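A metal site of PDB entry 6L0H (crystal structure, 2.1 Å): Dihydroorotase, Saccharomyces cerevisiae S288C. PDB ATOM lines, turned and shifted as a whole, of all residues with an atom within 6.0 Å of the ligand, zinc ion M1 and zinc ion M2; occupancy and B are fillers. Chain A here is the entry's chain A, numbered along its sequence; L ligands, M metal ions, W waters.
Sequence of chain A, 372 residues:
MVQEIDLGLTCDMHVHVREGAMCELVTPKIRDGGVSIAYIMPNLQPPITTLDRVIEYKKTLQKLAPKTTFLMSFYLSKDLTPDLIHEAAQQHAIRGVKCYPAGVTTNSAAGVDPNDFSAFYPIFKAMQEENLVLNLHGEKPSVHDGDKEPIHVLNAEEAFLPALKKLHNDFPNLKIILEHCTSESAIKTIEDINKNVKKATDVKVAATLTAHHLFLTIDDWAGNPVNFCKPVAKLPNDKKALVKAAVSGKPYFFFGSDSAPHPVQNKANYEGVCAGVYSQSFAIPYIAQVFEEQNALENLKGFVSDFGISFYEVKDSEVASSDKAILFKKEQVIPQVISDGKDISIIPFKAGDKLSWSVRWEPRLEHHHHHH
O5 of the ligand binds zinc ion M1 (1.9 Å). The side-chain carboxylate (OD1) of Asp 258 is bound to zinc ion M1 (2.0 Å). NE2 of His 14 is bound to zinc ion M1 (2.0 Å). Zinc ion M1 is bound by a ring nitrogen (NE2) of His 16 (2.0 Å). OQ1 of KCX 98 binds zinc ion M1, 2.2 Å away. Zinc ion M1 has five donor atoms within binding distance.
An oxygen (O2) of the ligand is in salt-bridge range of the guanidinium group of Arg 18 (2.8 Å). The backbone carbonyl oxygen (O) of Ala 275 lies within hydrogen-bond range of an oxygen (O3) of the ligand. An oxygen (O1) of the ligand is in hydrogen-bond range of the side-chain hydroxyl (OG1) of Thr 106 (2.6 Å). OG1 of Thr 105 lies within hydrogen-bond range of O4 of the ligand (2.7 Å). An oxygen (O1) of the ligand sits at hydrogen-bond distance from a ring nitrogen (NE2) of His 262, 3.2 Å away. ND2 of Asn 43 lies within hydrogen-bond range of O2 of the ligand, at 2.9 Å.
The backbone carbonyl oxygen of Lys 230 sits close to an oxygen (O4) of the ligand (3.5 Å). Merely in contact with the ligand: Ala 260. Hydrophobic or aromatic side chains within 4 Å of the ligand: His 16, His 137, His 180, Ala 260 and His 262. The nearest printed residue that does not touch the ligand is Gly 276 (4.1 Å).
Water W1 lies within hydrogen-bond range of O3 of the ligand (2.8 Å), N of Lys 230 (3.0 Å) and OD2 of Asp 258 (3.3 Å).
Zinc ion M2 is bound by OQ2 of KCX 98 (2.0 Å), a ring nitrogen (ND1) of His 137 (2.1 Å), a ring nitrogen (NE2) of His 180 (2.1 Å) and an oxygen (O5) of the ligand (2.4 Å). Zinc ion M2 has four donor atoms within binding distance. Slightly farther from zinc ion M2 lies an oxygen (O4) of the ligand (2.8 Å).
The backbone carbonyl oxygen of Ala 275 is in hydrogen-bond range of a ring nitrogen (NE2) of His 262, 2.7 Å away. ND1 of His 16 sits at hydrogen-bond distance from OD1 of Asn 43. NZ of KCX 98 is in hydrogen-bond range of the side-chain hydroxyl (OH) of Tyr 100 (3.0 Å). The side-chain hydroxyl (OG1) of Thr 106 is in hydrogen-bond range of the backbone carbonyl oxygen (O) of Ala 275, 3.3 Å away. The backbone carbonyl oxygen (O) of Thr 106 lies within hydrogen-bond range of the side-chain amide nitrogen (ND2) of Asn 43, at 3.1 Å. NH2 of Arg 18 sits close to NE2 of His 262 (3.4 Å). The side-chain carboxylate (OE1) of Glu 179 lies within hydrogen-bond range of a ring nitrogen (ND1) of His 14, 2.9 Å away. NE of Arg 18 lies within hydrogen-bond range of O of Pro 261, 2.9 Å away.
Of the 22 residues printed, 3 come within 4 Å of zinc ion M2. Along chain A the residues within 4 Å of zinc ion M2 span positions 98 to 180.
Four residues have an atom within 4 Å of zinc ion M1: His 14, His 16, KCX 98 and Asp 258.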
ATOM      1  N   HIS A  14      22.316   8.443   7.269  1.00  0.00           N
ATOM      2  CA  HIS A  14      22.027   8.996   5.932  1.00  0.00           C
ATOM      3  C   HIS A  14      22.667  10.390   5.849  1.00  0.00           C
ATOM      4  O   HIS A  14      22.046  11.374   6.237  1.00  0.00           O
ATOM      5  CB  HIS A  14      20.538   9.018   5.676  1.00  0.00           C
ATOM      6  CG  HIS A  14      20.169   9.312   4.262  1.00  0.00           C
ATOM      7  ND1 HIS A  14      19.156   8.644   3.598  1.00  0.00           N
ATOM      8  CD2 HIS A  14      20.651  10.222   3.382  1.00  0.00           C
ATOM      9  CE1 HIS A  14      19.047   9.135   2.374  1.00  0.00           C
ATOM     10  NE2 HIS A  14      19.946  10.094   2.223  1.00  0.00           N
ATOM     11  N   HIS A  16      25.097  13.240   3.559  1.00  0.00           N
ATOM     12  CA  HIS A  16      25.753  13.781   2.368  1.00  0.00           C
ATOM     13  C   HIS A  16      26.842  14.744   2.809  1.00  0.00           C
ATOM     14  O   HIS A  16      26.581  15.672   3.576  1.00  0.00           O
ATOM     15  CB  HIS A  16      24.765  14.496   1.446  1.00  0.00           C
ATOM     16  CG  HIS A  16      23.709  13.583   0.923  1.00  0.00           C
ATOM     17  ND1 HIS A  16      23.889  12.822  -0.202  1.00  0.00           N
ATOM     18  CD2 HIS A  16      22.477  13.286   1.391  1.00  0.00           C
ATOM     19  CE1 HIS A  16      22.803  12.095  -0.420  1.00  0.00           C
ATOM     20  NE2 HIS A  16      21.932  12.352   0.546  1.00  0.00           N
ATOM     21  N   ARG A  18      29.459  15.688   0.231  1.00  0.00           N
ATOM     22  CA  ARG A  18      29.965  16.313  -1.003  1.00  0.00           C
ATOM     23  C   ARG A  18      31.477  16.083  -1.145  1.00  0.00           C
ATOM     24  O   ARG A  18      32.023  15.092  -0.645  1.00  0.00           O
ATOM     25  CB  ARG A  18      29.571  17.791  -1.054  1.00  0.00           C
ATOM     26  CG  ARG A  18      28.133  18.116  -0.680  1.00  0.00           C
ATOM     27  CD  ARG A  18      27.105  17.377  -1.516  1.00  0.00           C
ATOM     28  NE  ARG A  18      25.781  17.917  -1.205  1.00  0.00           N
ATOM     29  CZ  ARG A  18      24.625  17.314  -1.464  1.00  0.00           C
ATOM     30  NH1 ARG A  18      24.592  16.104  -2.062  1.00  0.00           N
ATOM     31  NH2 ARG A  18      23.497  17.930  -1.143  1.00  0.00           N
ATOM     32  N   MET A  41      26.489   8.717   1.889  1.00  0.00           N
ATOM     33  CA  MET A  41      25.797   8.469   0.630  1.00  0.00           C
ATOM     34  C   MET A  41      26.704   8.755  -0.560  1.00  0.00           C
ATOM     35  O   MET A  41      27.647   9.549  -0.468  1.00  0.00           O
ATOM     36  CB  MET A  41      24.520   9.295   0.558  1.00  0.00           C
ATOM     37  CG  MET A  41      23.417   8.736   1.436  1.00  0.00           C
ATOM     38  SD  MET A  41      23.083   6.948   1.181  1.00  0.00           S
ATOM     39  CE  MET A  41      21.891   6.608   2.486  1.00  0.00           C
ATOM     40  N   ASN A  43      26.129   9.818  -3.966  1.00  0.00           N
ATOM     41  CA  ASN A  43      25.744  10.566  -5.169  1.00  0.00           C
ATOM     42  C   ASN A  43      26.663  11.776  -5.402  1.00  0.00           C
ATOM     43  O   ASN A  43      26.230  12.930  -5.425  1.00  0.00           O
ATOM     44  CB  ASN A  43      24.288  10.987  -5.082  1.00  0.00           C
ATOM     45  CG  ASN A  43      24.032  11.929  -3.932  1.00  0.00           C
ATOM     46  OD1 ASN A  43      24.754  11.922  -2.931  1.00  0.00           O
ATOM     47  ND2 ASN A  43      22.988  12.763  -4.064  1.00  0.00           N
ATOM     48  N   KCX A  98      23.443   2.171  -2.615  1.00  0.00           N
ATOM     49  CA  KCX A  98      22.313   3.091  -2.553  1.00  0.00           C
ATOM     50  CB  KCX A  98      22.778   4.466  -2.035  1.00  0.00           C
ATOM     51  CG  KCX A  98      21.733   5.569  -2.172  1.00  0.00           C
ATOM     52  CD  KCX A  98      20.553   5.316  -1.229  1.00  0.00           C
ATOM     53  CE  KCX A  98      19.617   6.514  -1.159  1.00  0.00           C
ATOM     54  NZ  KCX A  98      20.409   7.735  -0.925  1.00  0.00           N
ATOM     55  C   KCX A  98      21.662   3.237  -3.912  1.00  0.00           C
ATOM     56  O   KCX A  98      22.338   3.494  -4.911  1.00  0.00           O
ATOM     57  CX  KCX A  98      19.823   8.929  -0.787  1.00  0.00           C
ATOM     58  OQ1 KCX A  98      20.524   9.938  -0.613  1.00  0.00           O
ATOM     59  OQ2 KCX A  98      18.584   9.006  -0.836  1.00  0.00           O
ATOM     60  N   TYR A 100      19.250   5.253  -6.417  1.00  0.00           N
ATOM     61  CA  TYR A 100      18.540   6.486  -6.781  1.00  0.00           C
ATOM     62  C   TYR A 100      17.734   6.222  -8.040  1.00  0.00           C
ATOM     63  O   TYR A 100      18.336   5.910  -9.074  1.00  0.00           O
ATOM     64  CB  TYR A 100      19.505   7.651  -7.018  1.00  0.00           C
ATOM     65  CG  TYR A 100      20.276   8.114  -5.799  1.00  0.00           C
ATOM     66  CD1 TYR A 100      19.752   9.081  -4.949  1.00  0.00           C
ATOM     67  CD2 TYR A 100      21.517   7.593  -5.502  1.00  0.00           C
ATOM     68  CE1 TYR A 100      20.437   9.504  -3.847  1.00  0.00           C
ATOM     69  CE2 TYR A 100      22.234   8.024  -4.396  1.00  0.00           C
ATOM     70  CZ  TYR A 100      21.662   8.981  -3.568  1.00  0.00           C
ATOM     71  OH  TYR A 100      22.338   9.422  -2.454  1.00  0.00           O
ATOM     72  N   VAL A 104      14.851  11.822  -9.862  1.00  0.00           N
ATOM     73  CA  VAL A 104      14.002  12.246  -8.737  1.00  0.00           C
ATOM     74  C   VAL A 104      14.719  13.115  -7.707  1.00  0.00           C
ATOM     75  O   VAL A 104      14.031  13.695  -6.848  1.00  0.00           O
ATOM     76  CB  VAL A 104      13.325  11.069  -8.000  1.00  0.00           C
ATOM     77  CG1 VAL A 104      12.505  10.233  -8.976  1.00  0.00           C
ATOM     78  CG2 VAL A 104      14.361  10.200  -7.246  1.00  0.00           C
ATOM     79  N   THR A 105      16.060  13.216  -7.736  1.00  0.00           N
ATOM     80  CA  THR A 105      16.748  14.060  -6.742  1.00  0.00           C
ATOM     81  C   THR A 105      18.164  14.396  -7.213  1.00  0.00           C
ATOM     82  O   THR A 105      18.568  14.081  -8.339  1.00  0.00           O
ATOM     83  CB  THR A 105      16.779  13.415  -5.354  1.00  0.00           C
ATOM     84  OG1 THR A 105      17.206  14.380  -4.402  1.00  0.00           O
ATOM     85  CG2 THR A 105      17.710  12.197  -5.314  1.00  0.00           C
ATOM     86  N   THR A 106      18.938  15.039  -6.317  1.00  0.00           N
ATOM     87  CA  THR A 106      20.297  15.479  -6.631  1.00  0.00           C
ATOM     88  C   THR A 106      21.166  14.343  -7.188  1.00  0.00           C
ATOM     89  O   THR A 106      21.301  13.284  -6.580  1.00  0.00           O
ATOM     90  CB  THR A 106      20.971  16.061  -5.375  1.00  0.00           C
ATOM     91  OG1 THR A 106      20.212  17.178  -4.880  1.00  0.00           O
ATOM     92  CG2 THR A 106      22.396  16.535  -5.673  1.00  0.00           C
ATOM     93  N   HIS A 137      16.195   5.179  -2.161  1.00  0.00           N
ATOM     94  CA  HIS A 137      15.440   6.430  -2.262  1.00  0.00           C
ATOM     95  C   HIS A 137      14.148   6.029  -2.946  1.00  0.00           C
ATOM     96  O   HIS A 137      14.043   5.999  -4.175  1.00  0.00           O
ATOM     97  CB  HIS A 137      16.180   7.520  -3.032  1.00  0.00           C
ATOM     98  CG  HIS A 137      15.454   8.827  -3.091  1.00  0.00           C
ATOM     99  ND1 HIS A 137      15.975  10.011  -2.596  1.00  0.00           N
ATOM    100  CD2 HIS A 137      14.227   9.133  -3.586  1.00  0.00           C
ATOM    101  CE1 HIS A 137      15.102  10.980  -2.771  1.00  0.00           C
ATOM    102  NE2 HIS A 137      14.026  10.485  -3.372  1.00  0.00           N
ATOM    103  N   GLU A 179      14.823   4.685   2.785  1.00  0.00           N
ATOM    104  CA  GLU A 179      15.422   5.880   3.363  1.00  0.00           C
ATOM    105  C   GLU A 179      14.386   6.999   3.490  1.00  0.00           C
ATOM    106  O   GLU A 179      13.376   7.020   2.783  1.00  0.00           O
ATOM    107  CB  GLU A 179      16.614   6.341   2.497  1.00  0.00           C
ATOM    108  CG  GLU A 179      17.807   5.355   2.448  1.00  0.00           C
ATOM    109  CD  GLU A 179      18.512   5.189   3.800  1.00  0.00           C
ATOM    110  OE1 GLU A 179      18.407   6.093   4.650  1.00  0.00           O
ATOM    111  OE2 GLU A 179      19.216   4.169   4.025  1.00  0.00           O
ATOM    112  N   HIS A 180      14.628   7.908   4.436  1.00  0.00           N
ATOM    113  CA  HIS A 180      13.852   9.120   4.714  1.00  0.00           C
ATOM    114  C   HIS A 180      12.372   9.009   4.341  1.00  0.00           C
ATOM    115  O   HIS A 180      11.909   9.633   3.377  1.00  0.00           O
ATOM    116  CB  HIS A 180      14.487  10.350   4.031  1.00  0.00           C
ATOM    117  CG  HIS A 180      14.889  10.138   2.603  1.00  0.00           C
ATOM    118  ND1 HIS A 180      14.083   9.510   1.680  1.00  0.00           N
ATOM    119  CD2 HIS A 180      16.017  10.485   1.928  1.00  0.00           C
ATOM    120  CE1 HIS A 180      14.692   9.470   0.497  1.00  0.00           C
ATOM    121  NE2 HIS A 180      15.860  10.059   0.626  1.00  0.00           N
ATOM    122  N   CYS A 229      13.167  19.711  -0.228  1.00  0.00           N
ATOM    123  CA  CYS A 229      14.002  18.520  -0.281  1.00  0.00           C
ATOM    124  C   CYS A 229      13.214  17.405  -0.960  1.00  0.00           C
ATOM    125  O   CYS A 229      12.033  17.560  -1.264  1.00  0.00           O
ATOM    126  CB  CYS A 229      14.440  18.090   1.133  1.00  0.00           C
ATOM    127  SG  CYS A 229      13.031  17.572   2.159  1.00  0.00           S
ATOM    128  N   LYS A 230      13.909  16.305  -1.256  1.00  0.00           N
ATOM    129  CA  LYS A 230      13.297  15.058  -1.726  1.00  0.00           C
ATOM    130  C   LYS A 230      13.480  13.943  -0.690  1.00  0.00           C
ATOM    131  O   LYS A 230      14.566  13.824  -0.108  1.00  0.00           O
ATOM    132  CB  LYS A 230      13.918  14.608  -3.049  1.00  0.00           C
ATOM    133  CG  LYS A 230      13.710  15.581  -4.181  1.00  0.00           C
ATOM    134  CD  LYS A 230      12.242  15.949  -4.281  1.00  0.00           C
ATOM    135  CE  LYS A 230      11.748  15.816  -5.675  1.00  0.00           C
ATOM    136  NZ  LYS A 230      11.231  14.468  -6.018  1.00  0.00           N
ATOM    137  N   PRO A 231      12.457  13.100  -0.423  1.00  0.00           N
ATOM    138  CA  PRO A 231      11.066  13.296  -0.839  1.00  0.00           C
ATOM    139  C   PRO A 231      10.542  14.567  -0.179  1.00  0.00           C
ATOM    140  O   PRO A 231      11.017  14.973   0.887  1.00  0.00           O
ATOM    141  CB  PRO A 231      10.325  12.044  -0.329  1.00  0.00           C
ATOM    142  CG  PRO A 231      11.403  11.084   0.128  1.00  0.00           C
ATOM    143  CD  PRO A 231      12.582  11.958   0.491  1.00  0.00           C
ATOM    144  N   ASP A 258      19.556  12.696   6.282  1.00  0.00           N
ATOM    145  CA  ASP A 258      19.650  13.188   4.899  1.00  0.00           C
ATOM    146  C   ASP A 258      20.047  14.662   4.878  1.00  0.00           C
ATOM    147  O   ASP A 258      19.564  15.467   4.048  1.00  0.00           O
ATOM    148  CB  ASP A 258      18.367  12.961   4.110  1.00  0.00           C
ATOM    149  CG  ASP A 258      18.564  13.209   2.601  1.00  0.00           C
ATOM    150  OD1 ASP A 258      19.680  12.977   2.111  1.00  0.00           O
ATOM    151  OD2 ASP A 258      17.610  13.650   1.919  1.00  0.00           O
ATOM    152  N   ALA A 260      21.836  17.425   3.554  1.00  0.00           N
ATOM    153  CA  ALA A 260      22.220  17.544   2.157  1.00  0.00           C
ATOM    154  C   ALA A 260      22.660  18.985   1.926  1.00  0.00           C
ATOM    155  O   ALA A 260      21.834  19.849   1.598  1.00  0.00           O
ATOM    156  CB  ALA A 260      21.056  17.147   1.249  1.00  0.00           C
ATOM    157  N   PRO A 261      23.946  19.297   2.131  1.00  0.00           N
ATOM    158  CA  PRO A 261      24.381  20.696   2.034  1.00  0.00           C
ATOM    159  C   PRO A 261      24.458  21.191   0.601  1.00  0.00           C
ATOM    160  O   PRO A 261      24.862  20.469  -0.306  1.00  0.00           O
ATOM    161  CB  PRO A 261      25.749  20.713   2.721  1.00  0.00           C
ATOM    162  CG  PRO A 261      26.154  19.266   2.914  1.00  0.00           C
ATOM    163  CD  PRO A 261      25.027  18.375   2.511  1.00  0.00           C
ATOM    164  N   HIS A 262      23.985  22.429   0.387  1.00  0.00           N
ATOM    165  CA  HIS A 262      24.103  23.179  -0.863  1.00  0.00           C
ATOM    166  C   HIS A 262      24.528  24.606  -0.516  1.00  0.00           C
ATOM    167  O   HIS A 262      23.984  25.200   0.437  1.00  0.00           O
ATOM    168  CB  HIS A 262      22.789  23.249  -1.644  1.00  0.00           C
ATOM    169  CG  HIS A 262      22.246  21.918  -2.063  1.00  0.00           C
ATOM    170  ND1 HIS A 262      22.799  21.187  -3.101  1.00  0.00           N
ATOM    171  CD2 HIS A 262      21.199  21.191  -1.598  1.00  0.00           C
ATOM    172  CE1 HIS A 262      22.107  20.065  -3.252  1.00  0.00           C
ATOM    173  NE2 HIS A 262      21.139  20.047  -2.353  1.00  0.00           N
ATOM    174  N   ALA A 275      17.476  20.419  -4.366  1.00  0.00           N
ATOM    175  CA  ALA A 275      16.750  19.808  -3.254  1.00  0.00           C
ATOM    176  C   ALA A 275      17.720  19.412  -2.142  1.00  0.00           C
ATOM    177  O   ALA A 275      18.755  18.790  -2.396  1.00  0.00           O
ATOM    178  CB  ALA A 275      15.965  18.582  -3.730  1.00  0.00           C
ATOM    179  N   GLY A 276      17.373  19.736  -0.902  1.00  0.00           N
ATOM    180  CA  GLY A 276      18.173  19.344   0.241  1.00  0.00           C
ATOM    181  C   GLY A 276      18.138  20.351   1.376  1.00  0.00           C
ATOM    182  O   GLY A 276      18.130  21.572   1.156  1.00  0.00           O
HETATM  183  C1  LIG L   1      21.114  15.650  -2.103  1.00  0.00           C
HETATM  184  O1  LIG L   1      21.167  16.857  -2.436  1.00  0.00           O
HETATM  185  O2  LIG L   1      22.094  14.868  -2.252  1.00  0.00           O
HETATM  186  C2  LIG L   1      19.810  15.110  -1.518  1.00  0.00           C
HETATM  187  O3  LIG L   1      18.768  15.916  -1.983  1.00  0.00           O
HETATM  188  C3  LIG L   1      19.726  13.691  -2.048  1.00  0.00           C
HETATM  189  C4  LIG L   1      18.537  12.964  -1.435  1.00  0.00           C
HETATM  190  O4  LIG L   1      17.416  13.075  -1.996  1.00  0.00           O
HETATM  191  O5  LIG L   1      18.704  12.244  -0.407  1.00  0.00           O
HETATM  192 ZN    ZN M   1      20.065  11.543   0.794  1.00  0.00          ZN
HETATM  193 ZN    ZN M   2      17.201  10.500  -0.968  1.00  0.00          ZN
HETATM  194  O   HOH W   1      16.675  15.975  -0.184  1.00  0.00           O
